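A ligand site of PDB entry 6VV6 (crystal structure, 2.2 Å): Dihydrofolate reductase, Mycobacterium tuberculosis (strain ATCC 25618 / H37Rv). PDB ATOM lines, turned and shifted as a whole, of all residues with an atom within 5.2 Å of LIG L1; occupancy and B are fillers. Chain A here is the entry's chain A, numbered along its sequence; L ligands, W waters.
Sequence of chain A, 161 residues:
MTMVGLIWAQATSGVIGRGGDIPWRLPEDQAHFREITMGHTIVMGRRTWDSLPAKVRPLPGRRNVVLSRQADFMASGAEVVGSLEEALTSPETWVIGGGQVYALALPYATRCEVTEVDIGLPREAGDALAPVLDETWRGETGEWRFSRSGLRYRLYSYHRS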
ATOM      1  N   ILE A   7      10.900  -2.665   2.250  1.00  0.00           N
ATOM      2  CA  ILE A   7      11.351  -2.260   3.575  1.00  0.00           C
ATOM      3  C   ILE A   7      12.275  -3.348   4.136  1.00  0.00           C
ATOM      4  O   ILE A   7      11.915  -4.525   4.165  1.00  0.00           O
ATOM      5  CB  ILE A   7      10.165  -1.964   4.512  1.00  0.00           C
ATOM      6  CG1 ILE A   7      10.635  -1.562   5.904  1.00  0.00           C
ATOM      7  CG2 ILE A   7       9.188  -3.145   4.569  1.00  0.00           C
ATOM      8  CD1 ILE A   7       9.521  -1.032   6.779  1.00  0.00           C
ATOM      9  N   TRP A   8      13.480  -2.948   4.557  1.00  0.00           N
ATOM     10  CA  TRP A   8      14.458  -3.898   5.089  1.00  0.00           C
ATOM     11  C   TRP A   8      15.460  -3.204   6.010  1.00  0.00           C
ATOM     12  O   TRP A   8      15.640  -1.993   5.958  1.00  0.00           O
ATOM     13  CB  TRP A   8      15.200  -4.642   3.973  1.00  0.00           C
ATOM     14  CG  TRP A   8      16.249  -3.886   3.238  1.00  0.00           C
ATOM     15  CD1 TRP A   8      17.553  -3.765   3.591  1.00  0.00           C
ATOM     16  CD2 TRP A   8      16.112  -3.201   1.976  1.00  0.00           C
ATOM     17  NE1 TRP A   8      18.228  -3.015   2.665  1.00  0.00           N
ATOM     18  CE2 TRP A   8      17.365  -2.664   1.655  1.00  0.00           C
ATOM     19  CE3 TRP A   8      15.036  -2.977   1.100  1.00  0.00           C
ATOM     20  CZ2 TRP A   8      17.593  -1.916   0.495  1.00  0.00           C
ATOM     21  CZ3 TRP A   8      15.262  -2.235  -0.039  1.00  0.00           C
ATOM     22  CH2 TRP A   8      16.518  -1.712  -0.331  1.00  0.00           C
ATOM     23  N   ALA A   9      16.093  -4.005   6.846  1.00  0.00           N
ATOM     24  CA  ALA A   9      17.222  -3.578   7.651  1.00  0.00           C
ATOM     25  C   ALA A   9      18.469  -4.272   7.128  1.00  0.00           C
ATOM     26  O   ALA A   9      18.407  -5.402   6.644  1.00  0.00           O
ATOM     27  CB  ALA A   9      17.024  -3.897   9.140  1.00  0.00           C
ATOM     28  N   GLN A  10      19.602  -3.599   7.226  1.00  0.00           N
ATOM     29  CA  GLN A  10      20.807  -4.186   6.687  1.00  0.00           C
ATOM     30  C   GLN A  10      22.017  -3.687   7.463  1.00  0.00           C
ATOM     31  O   GLN A  10      21.997  -2.591   8.018  1.00  0.00           O
ATOM     32  CB  GLN A  10      20.964  -3.877   5.198  1.00  0.00           C
ATOM     33  CG  GLN A  10      21.130  -2.407   4.880  1.00  0.00           C
ATOM     34  CD  GLN A  10      21.686  -2.191   3.499  1.00  0.00           C
ATOM     35  OE1 GLN A  10      20.964  -2.274   2.517  1.00  0.00           O
ATOM     36  NE2 GLN A  10      22.970  -1.933   3.417  1.00  0.00           N
ATOM     37  N   ILE A  16      21.229  -8.824   5.038  1.00  0.00           N
ATOM     38  CA  ILE A  16      19.936  -8.721   5.706  1.00  0.00           C
ATOM     39  C   ILE A  16      19.535 -10.026   6.382  1.00  0.00           C
ATOM     40  O   ILE A  16      18.577 -10.019   7.175  1.00  0.00           O
ATOM     41  CB  ILE A  16      18.831  -8.265   4.733  1.00  0.00           C
ATOM     42  CG1 ILE A  16      18.548  -9.346   3.700  1.00  0.00           C
ATOM     43  CG2 ILE A  16      19.225  -6.982   4.026  1.00  0.00           C
ATOM     44  CD1 ILE A  16      17.264  -9.181   3.042  1.00  0.00           C
ATOM     45  N   GLY A  17      20.230 -11.123   6.124  1.00  0.00           N
ATOM     46  CA  GLY A  17      19.842 -12.391   6.696  1.00  0.00           C
ATOM     47  C   GLY A  17      20.841 -13.497   6.502  1.00  0.00           C
ATOM     48  O   GLY A  17      21.528 -13.539   5.479  1.00  0.00           O
ATOM     49  N   ARG A  18      20.926 -14.397   7.469  1.00  0.00           N
ATOM     50  CA  ARG A  18      21.915 -15.479   7.486  1.00  0.00           C
ATOM     51  C   ARG A  18      21.299 -16.686   8.192  1.00  0.00           C
ATOM     52  O   ARG A  18      20.679 -16.544   9.242  1.00  0.00           O
ATOM     53  CB  ARG A  18      23.208 -15.013   8.186  1.00  0.00           C
ATOM     54  CG  ARG A  18      24.279 -16.083   8.326  1.00  0.00           C
ATOM     55  CD  ARG A  18      25.554 -15.534   8.952  1.00  0.00           C
ATOM     56  NE  ARG A  18      26.172 -14.538   8.091  1.00  0.00           N
ATOM     57  CZ  ARG A  18      27.263 -13.838   8.420  1.00  0.00           C
ATOM     58  NH1 ARG A  18      27.835 -14.030   9.586  1.00  0.00           N
ATOM     59  NH2 ARG A  18      27.771 -12.951   7.574  1.00  0.00           N
ATOM     60  N   GLY A  19      21.449 -17.864   7.588  1.00  0.00           N
ATOM     61  CA  GLY A  19      20.897 -19.063   8.185  1.00  0.00           C
ATOM     62  C   GLY A  19      19.395 -19.062   8.283  1.00  0.00           C
ATOM     63  O   GLY A  19      18.840 -19.806   9.084  1.00  0.00           O
ATOM     64  N   GLY A  20      18.720 -18.234   7.490  1.00  0.00           N
ATOM     65  CA  GLY A  20      17.280 -18.126   7.565  1.00  0.00           C
ATOM     66  C   GLY A  20      16.741 -17.234   8.654  1.00  0.00           C
ATOM     67  O   GLY A  20      15.579 -17.376   9.029  1.00  0.00           O
ATOM     68  N   ASP A  21      17.540 -16.300   9.172  1.00  0.00           N
ATOM     69  CA  ASP A  21      17.064 -15.334  10.164  1.00  0.00           C
ATOM     70  C   ASP A  21      17.894 -14.056  10.025  1.00  0.00           C
ATOM     71  O   ASP A  21      18.431 -13.779   8.952  1.00  0.00           O
ATOM     72  CB  ASP A  21      17.107 -15.935  11.579  1.00  0.00           C
ATOM     73  CG  ASP A  21      16.000 -15.384  12.484  1.00  0.00           C
ATOM     74  OD1 ASP A  21      14.941 -16.042  12.583  1.00  0.00           O
ATOM     75  OD2 ASP A  21      16.190 -14.314  13.107  1.00  0.00           O
ATOM     76  N   ILE A  22      17.976 -13.278  11.110  1.00  0.00           N
ATOM     77  CA  ILE A  22      18.582 -11.963  11.115  1.00  0.00           C
ATOM     78  C   ILE A  22      19.605 -11.920  12.264  1.00  0.00           C
ATOM     79  O   ILE A  22      19.235 -12.145  13.419  1.00  0.00           O
ATOM     80  CB  ILE A  22      17.564 -10.830  11.294  1.00  0.00           C
ATOM     81  CG1 ILE A  22      16.398 -10.981  10.314  1.00  0.00           C
ATOM     82  CG2 ILE A  22      18.214  -9.460  11.124  1.00  0.00           C
ATOM     83  CD1 ILE A  22      15.343  -9.962  10.509  1.00  0.00           C
ATOM     84  N   TRP A  24      20.736  -9.640  14.020  1.00  0.00           N
ATOM     85  CA  TRP A  24      20.572  -8.556  14.975  1.00  0.00           C
ATOM     86  C   TRP A  24      19.092  -8.429  15.269  1.00  0.00           C
ATOM     87  O   TRP A  24      18.240  -8.938  14.533  1.00  0.00           O
ATOM     88  CB  TRP A  24      21.129  -7.231  14.455  1.00  0.00           C
ATOM     89  CG  TRP A  24      20.409  -6.779  13.255  1.00  0.00           C
ATOM     90  CD1 TRP A  24      19.188  -6.163  13.210  1.00  0.00           C
ATOM     91  CD2 TRP A  24      20.834  -6.950  11.914  1.00  0.00           C
ATOM     92  NE1 TRP A  24      18.827  -5.938  11.916  1.00  0.00           N
ATOM     93  CE2 TRP A  24      19.813  -6.409  11.098  1.00  0.00           C
ATOM     94  CE3 TRP A  24      21.959  -7.503  11.325  1.00  0.00           C
ATOM     95  CZ2 TRP A  24      19.912  -6.403   9.716  1.00  0.00           C
ATOM     96  CZ3 TRP A  24      22.044  -7.507   9.957  1.00  0.00           C
ATOM     97  CH2 TRP A  24      21.023  -6.958   9.162  1.00  0.00           C
ATOM     98  N   GLY A  45       8.394 -13.689   0.932  1.00  0.00           N
ATOM     99  CA  GLY A  45       8.657 -15.020   0.427  1.00  0.00           C
ATOM    100  C   GLY A  45       8.387 -16.091   1.471  1.00  0.00           C
ATOM    101  O   GLY A  45       8.277 -15.814   2.660  1.00  0.00           O
ATOM    102  N   ARG A  46       8.258 -17.327   0.991  1.00  0.00           N
ATOM    103  CA  ARG A  46       7.949 -18.459   1.878  1.00  0.00           C
ATOM    104  C   ARG A  46       9.006 -18.627   2.958  1.00  0.00           C
ATOM    105  O   ARG A  46       8.681 -18.975   4.097  1.00  0.00           O
ATOM    106  CB  ARG A  46       7.809 -19.741   1.047  1.00  0.00           C
ATOM    107  CG  ARG A  46       7.290 -20.982   1.778  1.00  0.00           C
ATOM    108  CD  ARG A  46       8.393 -21.870   2.342  1.00  0.00           C
ATOM    109  NE  ARG A  46       9.333 -22.370   1.359  1.00  0.00           N
ATOM    110  CZ  ARG A  46      10.519 -22.902   1.655  1.00  0.00           C
ATOM    111  NH1 ARG A  46      10.894 -22.985   2.909  1.00  0.00           N
ATOM    112  NH2 ARG A  46      11.321 -23.341   0.690  1.00  0.00           N
ATOM    113  N   ARG A  47      10.276 -18.389   2.620  1.00  0.00           N
ATOM    114  CA  ARG A  47      11.321 -18.504   3.633  1.00  0.00           C
ATOM    115  C   ARG A  47      11.164 -17.454   4.730  1.00  0.00           C
ATOM    116  O   ARG A  47      11.453 -17.728   5.895  1.00  0.00           O
ATOM    117  CB  ARG A  47      12.696 -18.424   2.961  1.00  0.00           C
ATOM    118  CG  ARG A  47      12.934 -19.552   1.963  1.00  0.00           C
ATOM    119  CD  ARG A  47      14.396 -19.664   1.530  1.00  0.00           C
ATOM    120  NE  ARG A  47      14.668 -20.984   0.992  1.00  0.00           N
ATOM    121  CZ  ARG A  47      15.773 -21.320   0.355  1.00  0.00           C
ATOM    122  NH1 ARG A  47      16.734 -20.433   0.156  1.00  0.00           N
ATOM    123  NH2 ARG A  47      15.916 -22.564  -0.094  1.00  0.00           N
ATOM    124  N   THR A  48      10.685 -16.246   4.386  1.00  0.00           N
ATOM    125  CA  THR A  48      10.493 -15.211   5.399  1.00  0.00           C
ATOM    126  C   THR A  48       9.249 -15.483   6.246  1.00  0.00           C
ATOM    127  O   THR A  48       9.274 -15.323   7.467  1.00  0.00           O
ATOM    128  CB  THR A  48      10.422 -13.833   4.757  1.00  0.00           C
ATOM    129  OG1 THR A  48      11.738 -13.409   4.425  1.00  0.00           O
ATOM    130  CG2 THR A  48       9.800 -12.812   5.718  1.00  0.00           C
ATOM    131  N   SER A  51      10.157 -17.796   8.628  1.00  0.00           N
ATOM    132  CA  SER A  51      10.921 -17.228   9.731  1.00  0.00           C
ATOM    133  C   SER A  51      10.045 -16.559  10.797  1.00  0.00           C
ATOM    134  O   SER A  51      10.553 -16.252  11.875  1.00  0.00           O
ATOM    135  CB  SER A  51      11.936 -16.206   9.202  1.00  0.00           C
ATOM    136  OG  SER A  51      11.299 -15.024   8.785  1.00  0.00           O
ATOM    137  N   LEU A  67       4.665 -15.605  -1.157  1.00  0.00           N
ATOM    138  CA  LEU A  67       5.013 -15.962  -2.526  1.00  0.00           C
ATOM    139  C   LEU A  67       5.765 -17.294  -2.529  1.00  0.00           C
ATOM    140  O   LEU A  67       6.663 -17.500  -1.709  1.00  0.00           O
ATOM    141  CB  LEU A  67       5.872 -14.856  -3.156  1.00  0.00           C
ATOM    142  CG  LEU A  67       6.129 -14.803  -4.651  1.00  0.00           C
ATOM    143  CD1 LEU A  67       4.900 -14.325  -5.352  1.00  0.00           C
ATOM    144  CD2 LEU A  67       7.262 -13.848  -4.903  1.00  0.00           C
ATOM    145  N   SER A  68       5.398 -18.200  -3.440  1.00  0.00           N
ATOM    146  CA  SER A  68       5.866 -19.583  -3.370  1.00  0.00           C
ATOM    147  C   SER A  68       5.641 -20.300  -4.705  1.00  0.00           C
ATOM    148  O   SER A  68       4.643 -20.047  -5.383  1.00  0.00           O
ATOM    149  CB  SER A  68       5.160 -20.331  -2.228  1.00  0.00           C
ATOM    150  OG  SER A  68       5.628 -21.668  -2.094  1.00  0.00           O
ATOM    151  N   ARG A  69       6.584 -21.191  -5.051  1.00  0.00           N
ATOM    152  CA  ARG A  69       6.452 -22.075  -6.210  1.00  0.00           C
ATOM    153  C   ARG A  69       5.759 -23.392  -5.892  1.00  0.00           C
ATOM    154  O   ARG A  69       5.433 -24.148  -6.808  1.00  0.00           O
ATOM    155  CB  ARG A  69       7.820 -22.373  -6.843  1.00  0.00           C
ATOM    156  CG  ARG A  69       8.644 -21.140  -7.262  1.00  0.00           C
ATOM    157  CD  ARG A  69       9.672 -21.485  -8.335  1.00  0.00           C
ATOM    158  NE  ARG A  69      10.413 -20.327  -8.838  1.00  0.00           N
ATOM    159  CZ  ARG A  69      11.691 -20.070  -8.556  1.00  0.00           C
ATOM    160  NH1 ARG A  69      12.380 -20.879  -7.756  1.00  0.00           N
ATOM    161  NH2 ARG A  69      12.283 -19.003  -9.065  1.00  0.00           N
ATOM    162  N   GLN A  70       5.533 -23.711  -4.612  1.00  0.00           N
ATOM    163  CA  GLN A  70       4.717 -24.860  -4.254  1.00  0.00           C
ATOM    164  C   GLN A  70       3.261 -24.516  -4.507  1.00  0.00           C
ATOM    165  O   GLN A  70       2.702 -23.626  -3.848  1.00  0.00           O
ATOM    166  CB  GLN A  70       4.890 -25.239  -2.793  1.00  0.00           C
ATOM    167  CG  GLN A  70       6.288 -25.517  -2.377  1.00  0.00           C
ATOM    168  CD  GLN A  70       6.343 -25.931  -0.948  1.00  0.00           C
ATOM    169  OE1 GLN A  70       5.533 -26.748  -0.496  1.00  0.00           O
ATOM    170  NE2 GLN A  70       7.282 -25.365  -0.202  1.00  0.00           N
ATOM    171  N   GLY A  82       1.165 -17.259  -6.350  1.00  0.00           N
ATOM    172  CA  GLY A  82       2.262 -17.817  -7.118  1.00  0.00           C
ATOM    173  C   GLY A  82       3.041 -16.783  -7.905  1.00  0.00           C
ATOM    174  O   GLY A  82       4.147 -17.083  -8.355  1.00  0.00           O
ATOM    175  N   ILE A  96       8.205  -7.179   2.333  1.00  0.00           N
ATOM    176  CA  ILE A  96       8.944  -7.238   3.584  1.00  0.00           C
ATOM    177  C   ILE A  96      10.033  -8.312   3.543  1.00  0.00           C
ATOM    178  O   ILE A  96      10.464  -8.799   4.590  1.00  0.00           O
ATOM    179  CB  ILE A  96       8.001  -7.456   4.778  1.00  0.00           C
ATOM    180  CG1 ILE A  96       7.290  -8.812   4.686  1.00  0.00           C
ATOM    181  CG2 ILE A  96       6.999  -6.332   4.859  1.00  0.00           C
ATOM    182  CD1 ILE A  96       6.704  -9.317   5.981  1.00  0.00           C
ATOM    183  N   GLY A  97      10.486  -8.691   2.353  1.00  0.00           N
ATOM    184  CA  GLY A  97      11.602  -9.607   2.218  1.00  0.00           C
ATOM    185  C   GLY A  97      11.254 -11.014   1.841  1.00  0.00           C
ATOM    186  O   GLY A  97      10.096 -11.339   1.649  1.00  0.00           O
ATOM    187  N   GLY A  98      12.270 -11.873   1.725  1.00  0.00           N
ATOM    188  CA  GLY A  98      13.647 -11.483   1.954  1.00  0.00           C
ATOM    189  C   GLY A  98      14.402 -11.112   0.692  1.00  0.00           C
ATOM    190  O   GLY A  98      13.842 -10.481  -0.201  1.00  0.00           O
ATOM    191  N   GLY A  99      15.657 -11.550   0.622  1.00  0.00           N
ATOM    192  CA  GLY A  99      16.555 -11.072  -0.426  1.00  0.00           C
ATOM    193  C   GLY A  99      16.098 -11.420  -1.830  1.00  0.00           C
ATOM    194  O   GLY A  99      16.282 -10.644  -2.770  1.00  0.00           O
ATOM    195  N   GLN A 100      15.509 -12.605  -1.989  1.00  0.00           N
ATOM    196  CA  GLN A 100      15.001 -13.009  -3.299  1.00  0.00           C
ATOM    197  C   GLN A 100      13.781 -12.178  -3.699  1.00  0.00           C
ATOM    198  O   GLN A 100      13.633 -11.825  -4.878  1.00  0.00           O
ATOM    199  CB  GLN A 100      14.706 -14.521  -3.321  1.00  0.00           C
ATOM    200  CG  GLN A 100      15.963 -15.410  -3.440  1.00  0.00           C
ATOM    201  CD  GLN A 100      15.666 -16.907  -3.482  1.00  0.00           C
ATOM    202  OE1 GLN A 100      14.521 -17.328  -3.609  1.00  0.00           O
ATOM    203  NE2 GLN A 100      16.714 -17.708  -3.377  1.00  0.00           N
ATOM    204  N   VAL A 101      12.906 -11.844  -2.750  1.00  0.00           N
ATOM    205  CA  VAL A 101      11.720 -11.102  -3.131  1.00  0.00           C
ATOM    206  C   VAL A 101      12.012  -9.617  -3.285  1.00  0.00           C
ATOM    207  O   VAL A 101      11.350  -8.933  -4.077  1.00  0.00           O
ATOM    208  CB  VAL A 101      10.582 -11.369  -2.125  1.00  0.00           C
ATOM    209  CG1 VAL A 101       9.354 -10.525  -2.430  1.00  0.00           C
ATOM    210  CG2 VAL A 101      10.232 -12.829  -2.152  1.00  0.00           C
ATOM    211  N   TYR A 102      13.002  -9.089  -2.564  1.00  0.00           N
ATOM    212  CA  TYR A 102      13.350  -7.678  -2.715  1.00  0.00           C
ATOM    213  C   TYR A 102      13.718  -7.367  -4.157  1.00  0.00           C
ATOM    214  O   TYR A 102      13.259  -6.371  -4.731  1.00  0.00           O
ATOM    215  CB  TYR A 102      14.495  -7.288  -1.782  1.00  0.00           C
ATOM    216  CG  TYR A 102      14.098  -7.121  -0.335  1.00  0.00           C
ATOM    217  CD1 TYR A 102      12.871  -6.570   0.022  1.00  0.00           C
ATOM    218  CD2 TYR A 102      14.941  -7.532   0.689  1.00  0.00           C
ATOM    219  CE1 TYR A 102      12.502  -6.436   1.357  1.00  0.00           C
ATOM    220  CE2 TYR A 102      14.589  -7.410   2.019  1.00  0.00           C
ATOM    221  CZ  TYR A 102      13.370  -6.863   2.353  1.00  0.00           C
ATOM    222  OH  TYR A 102      13.035  -6.732   3.679  1.00  0.00           O
ATOM    223  N   LEU A 104      12.973  -9.326  -6.914  1.00  0.00           N
ATOM    224  CA  LEU A 104      11.820  -9.594  -7.778  1.00  0.00           C
ATOM    225  C   LEU A 104      10.776  -8.486  -7.665  1.00  0.00           C
ATOM    226  O   LEU A 104      10.121  -8.141  -8.659  1.00  0.00           O
ATOM    227  CB  LEU A 104      11.227 -10.967  -7.426  1.00  0.00           C
ATOM    228  CG  LEU A 104       9.769 -11.293  -7.736  1.00  0.00           C
ATOM    229  CD1 LEU A 104       9.475 -11.226  -9.229  1.00  0.00           C
ATOM    230  CD2 LEU A 104       9.479 -12.678  -7.237  1.00  0.00           C
ATOM    231  N   ALA A 128      21.476 -13.701   2.484  1.00  0.00           N
ATOM    232  CA  ALA A 128      20.560 -12.880   1.703  1.00  0.00           C
ATOM    233  C   ALA A 128      20.985 -11.409   1.772  1.00  0.00           C
ATOM    234  O   ALA A 128      21.444 -10.950   2.818  1.00  0.00           O
ATOM    235  CB  ALA A 128      19.135 -13.039   2.220  1.00  0.00           C
HETATM  236  P1  LIG L   1      12.866 -15.385   0.477  1.00  0.00           P
HETATM  237  O1  LIG L   1      12.450 -15.031   1.854  1.00  0.00           O
HETATM  238  O2  LIG L   1      13.157 -14.311  -0.521  1.00  0.00           O
HETATM  239  O3  LIG L   1      11.667 -16.395  -0.114  1.00  0.00           O
HETATM  240  C1  LIG L   1      12.264 -17.260  -1.051  1.00  0.00           C
HETATM  241  C2  LIG L   1      11.141 -18.151  -1.627  1.00  0.00           C
HETATM  242  O4  LIG L   1      10.226 -17.350  -2.357  1.00  0.00           O
HETATM  243  C3  LIG L   1      11.642 -19.248  -2.589  1.00  0.00           C
HETATM  244  O5  LIG L   1      12.193 -20.317  -1.908  1.00  0.00           O
HETATM  245  C4  LIG L   1      10.270 -19.637  -3.183  1.00  0.00           C
HETATM  246  O6  LIG L   1       9.476 -20.313  -2.326  1.00  0.00           O
HETATM  247  C5  LIG L   1       9.682 -18.167  -3.394  1.00  0.00           C
HETATM  248  N1  LIG L   1      10.085 -17.567  -4.679  1.00  0.00           N
HETATM  249  C6  LIG L   1      11.367 -17.142  -5.054  1.00  0.00           C
HETATM  250  N2  LIG L   1      11.418 -16.657  -6.311  1.00  0.00           N
HETATM  251  C7  LIG L   1      10.110 -16.772  -6.766  1.00  0.00           C
HETATM  252  C8  LIG L   1       9.513 -16.436  -7.982  1.00  0.00           C
HETATM  253  N3  LIG L   1      10.269 -15.880  -8.989  1.00  0.00           N
HETATM  254  N4  LIG L   1       8.186 -16.626  -8.207  1.00  0.00           N
HETATM  255  C9  LIG L   1       7.503 -17.186  -7.147  1.00  0.00           C
HETATM  256  N5  LIG L   1       7.912 -17.566  -5.935  1.00  0.00           N
HETATM  257  C10 LIG L   1       9.258 -17.345  -5.755  1.00  0.00           C
HETATM  258  O7  LIG L   1      14.227 -16.341   0.721  1.00  0.00           O
HETATM  259  P2  LIG L   1      15.587 -15.554   1.054  1.00  0.00           P
HETATM  260  O8  LIG L   1      16.468 -16.570   1.660  1.00  0.00           O
HETATM  261  O9  LIG L   1      16.140 -14.636  -0.020  1.00  0.00           O
HETATM  262  O10 LIG L   1      15.339 -14.347   2.347  1.00  0.00           O
HETATM  263  C11 LIG L   1      15.319 -14.922   3.613  1.00  0.00           C
HETATM  264  C12 LIG L   1      16.150 -14.040   4.577  1.00  0.00           C
HETATM  265  O11 LIG L   1      15.700 -12.650   4.646  1.00  0.00           O
HETATM  266  C13 LIG L   1      16.003 -14.604   5.981  1.00  0.00           C
HETATM  267  O12 LIG L   1      17.284 -14.826   6.440  1.00  0.00           O
HETATM  268  C14 LIG L   1      15.273 -13.457   6.747  1.00  0.00           C
HETATM  269  O13 LIG L   1      15.634 -13.351   8.053  1.00  0.00           O
HETATM  270  C15 LIG L   1      15.820 -12.232   5.997  1.00  0.00           C
HETATM  271  N6  LIG L   1      14.985 -11.025   6.183  1.00  0.00           N
HETATM  272  C16 LIG L   1      15.551  -9.894   6.699  1.00  0.00           C
HETATM  273  C17 LIG L   1      14.867  -8.721   6.698  1.00  0.00           C
HETATM  274  C18 LIG L   1      15.543  -7.583   7.246  1.00  0.00           C
HETATM  275  O14 LIG L   1      16.704  -7.596   7.663  1.00  0.00           O
HETATM  276  N7  LIG L   1      14.798  -6.427   7.292  1.00  0.00           N
HETATM  277  C19 LIG L   1      13.480  -8.590   6.170  1.00  0.00           C
HETATM  278  C20 LIG L   1      12.924  -9.896   5.759  1.00  0.00           C
HETATM  279  C21 LIG L   1      13.636 -11.010   5.775  1.00  0.00           C
HETATM  280  P3  LIG L   1       9.305 -22.127  -2.662  1.00  0.00           P
HETATM  281  O15 LIG L   1       8.867 -21.966  -4.082  1.00  0.00           O
HETATM  282  O16 LIG L   1      10.699 -22.704  -2.443  1.00  0.00           O
HETATM  283  O17 LIG L   1       8.244 -22.466  -1.659  1.00  0.00           O
HETATM  284  C1  LG2 L   2      10.532 -10.673  15.732  1.00  0.00           C
HETATM  285  C2  LG2 L   2       9.139 -12.575  15.365  1.00  0.00           C
HETATM  286  C3  LG2 L   2       6.568  -9.099  14.380  1.00  0.00           C
HETATM  287  C4  LG2 L   2       7.666  -8.048  12.608  1.00  0.00           C
HETATM  288  C5  LG2 L   2      10.837  -7.579  11.258  1.00  0.00           C
HETATM  289  C6  LG2 L   2      12.211  -7.411  11.180  1.00  0.00           C
HETATM  290  C7  LG2 L   2      11.580  -9.764   8.584  1.00  0.00           C
HETATM  291  C8  LG2 L   2       9.202  -9.970   8.813  1.00  0.00           C
HETATM  292  C9  LG2 L   2      10.475  -8.503  10.272  1.00  0.00           C
HETATM  293  O1  LG2 L   2       3.277  -7.430  14.179  1.00  0.00           O
HETATM  294  C10 LG2 L   2       4.491  -7.535  13.863  1.00  0.00           C
HETATM  295  O2  LG2 L   2       4.908  -6.938  12.823  1.00  0.00           O
HETATM  296  C11 LG2 L   2       5.440  -8.370  14.749  1.00  0.00           C
HETATM  297  C12 LG2 L   2       5.327  -8.519  16.119  1.00  0.00           C
HETATM  298  N1  LG2 L   2       6.307  -9.290  16.554  1.00  0.00           N
HETATM  299  N2  LG2 L   2       7.075  -9.635  15.477  1.00  0.00           N
HETATM  300  C13 LG2 L   2       8.158 -10.404  15.512  1.00  0.00           C
HETATM  301  C14 LG2 L   2       9.412  -9.857  15.709  1.00  0.00           C
HETATM  302  C15 LG2 L   2      10.386 -12.041  15.552  1.00  0.00           C
HETATM  303  F1  LG2 L   2      11.456 -12.873  15.577  1.00  0.00           F
HETATM  304  C16 LG2 L   2       8.024 -11.768  15.340  1.00  0.00           C
HETATM  305  O3  LG2 L   2       7.107  -9.242  13.093  1.00  0.00           O
HETATM  306  C17 LG2 L   2       9.121  -7.944  13.055  1.00  0.00           C
HETATM  307  C18 LG2 L   2       9.888  -6.900  12.240  1.00  0.00           C
HETATM  308  N3  LG2 L   2      12.653  -8.170  10.205  1.00  0.00           N
HETATM  309  C19 LG2 L   2      11.631  -8.846   9.632  1.00  0.00           C
HETATM  310  C20 LG2 L   2      10.382 -10.312   8.177  1.00  0.00           C
HETATM  311  C21 LG2 L   2       9.253  -9.075   9.859  1.00  0.00           C
HETATM  312  O   HOH W   1      13.221 -12.362   9.011  1.00  0.00           O
HETATM  313  O   HOH W   2      19.258 -14.453  -0.963  1.00  0.00           O
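NE of Arg 46 lies within salt-bridge range of O17 of LIG L1 (3.2 Å). The backbone NH (N) of Gly 98 is in hydrogen-bond range of an oxygen (O1) of LIG L1 (3.2 Å). The side-chain hydroxyl (OG1) of Thr 48 is in hydrogen-bond range of an oxygen (O1) of LIG L1, at 3.1 Å. The side-chain amide nitrogen (NE2) of Gln 70 sits at hydrogen-bond distance from an oxygen (O17) of LIG L1 (3.4 Å). An oxygen (O15) of LIG L1 is in hydrogen-bond range of the backbone NH (N) of Arg 69 (2.6 Å). An oxygen (O9) of LIG L1 is in hydrogen-bond range of the backbone NH of Gln 100 (2.9 Å). The side-chain hydroxyl (OG) of Ser 68 lies within hydrogen-bond range of an oxygen (O17) of LIG L1 (2.8 Å). The backbone NH (N) of Val 101 sits at hydrogen-bond distance from an oxygen (O2) of LIG L1 (3.3 Å). N of Thr 48 sits at hydrogen-bond distance from O1 of LIG L1. The backbone NH (N) of Gly 99 is in hydrogen-bond range of an oxygen (O9) of LIG L1, 3.2 Å away. The backbone NH (N) of Asp 21 sits at hydrogen-bond distance from an oxygen (O12) of LIG L1, 3.1 Å away. The backbone carbonyl oxygen (O) of Asp 21 sits at hydrogen-bond distance from an oxygen (O12) of LIG L1, at 3.0 Å.
OH of Tyr 102 sits at hydrogen-bond distance from O of Ile 7 (2.5 Å). OE1 of Gln 10 lies within hydrogen-bond range of NE1 of Trp 8 (2.8 Å). N of Gly 97 lies close to OH of Tyr 102, 3.5 Å away. OG of Ser 68 lies within hydrogen-bond range of N of Gln 70, 3.2 Å away. N of Gly 98 is in hydrogen-bond range of OG1 of Thr 48 (3.2 Å). O of Thr 48 sits at hydrogen-bond distance from OG of Ser 51 (2.4 Å). O of Gly 97 lies within hydrogen-bond range of N of Gly 45. O of Ile 96 lies close to OH of Tyr 102.
Water W1 lies within hydrogen-bond range of O13 of LIG L1 (2.8 Å) and OG of Ser 51 (3.3 Å).
N of Ala 9 sits close to N7 of LIG L1 (2.8 Å). An oxygen (O14) of LIG L1 lies close to the backbone carbonyl oxygen of Ile 16, at 3.1 Å. Residues that only touch LIG L1: Trp 8 (3.4 Å), Gly 17 (3.5 Å), Arg 18 (3.8 Å), Gly 20 (3.3 Å), Ile 22 (3.4 Å), Trp 24 (3.99 Å), Gly 45 (3.4 Å), Arg 47 (3.4 Å), Leu 67 (3.5 Å), Gly 82 (3.6 Å), Ile 96 (2.9 Å), Gly 97 (3.8 Å), Tyr 102 (3.1 Å), Leu 104 (3.7 Å) and Ala 128 (3.9 Å). Hydrophobic or aromatic side chains within 4 Å of LIG L1: Trp 8, Ala 9, Ile 16, Ile 22, Trp 24, Leu 67, Val 101, Leu 104 and Ala 128. Within 4 Å of LIG L1: Trp 8, Ala 9, Ile 16, Gly 17, Arg 18, Gly 20, Asp 21, Ile 22, Trp 24, Gly 45, Arg 46, Arg 47, Thr 48, Leu 67, Ser 68, Arg 69, Gln 70, Gly 82, Ile 96, Gly 97, Gly 98, Gly 99, Gln 100, Val 101, Tyr 102, Leu 104 and Ala 128.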
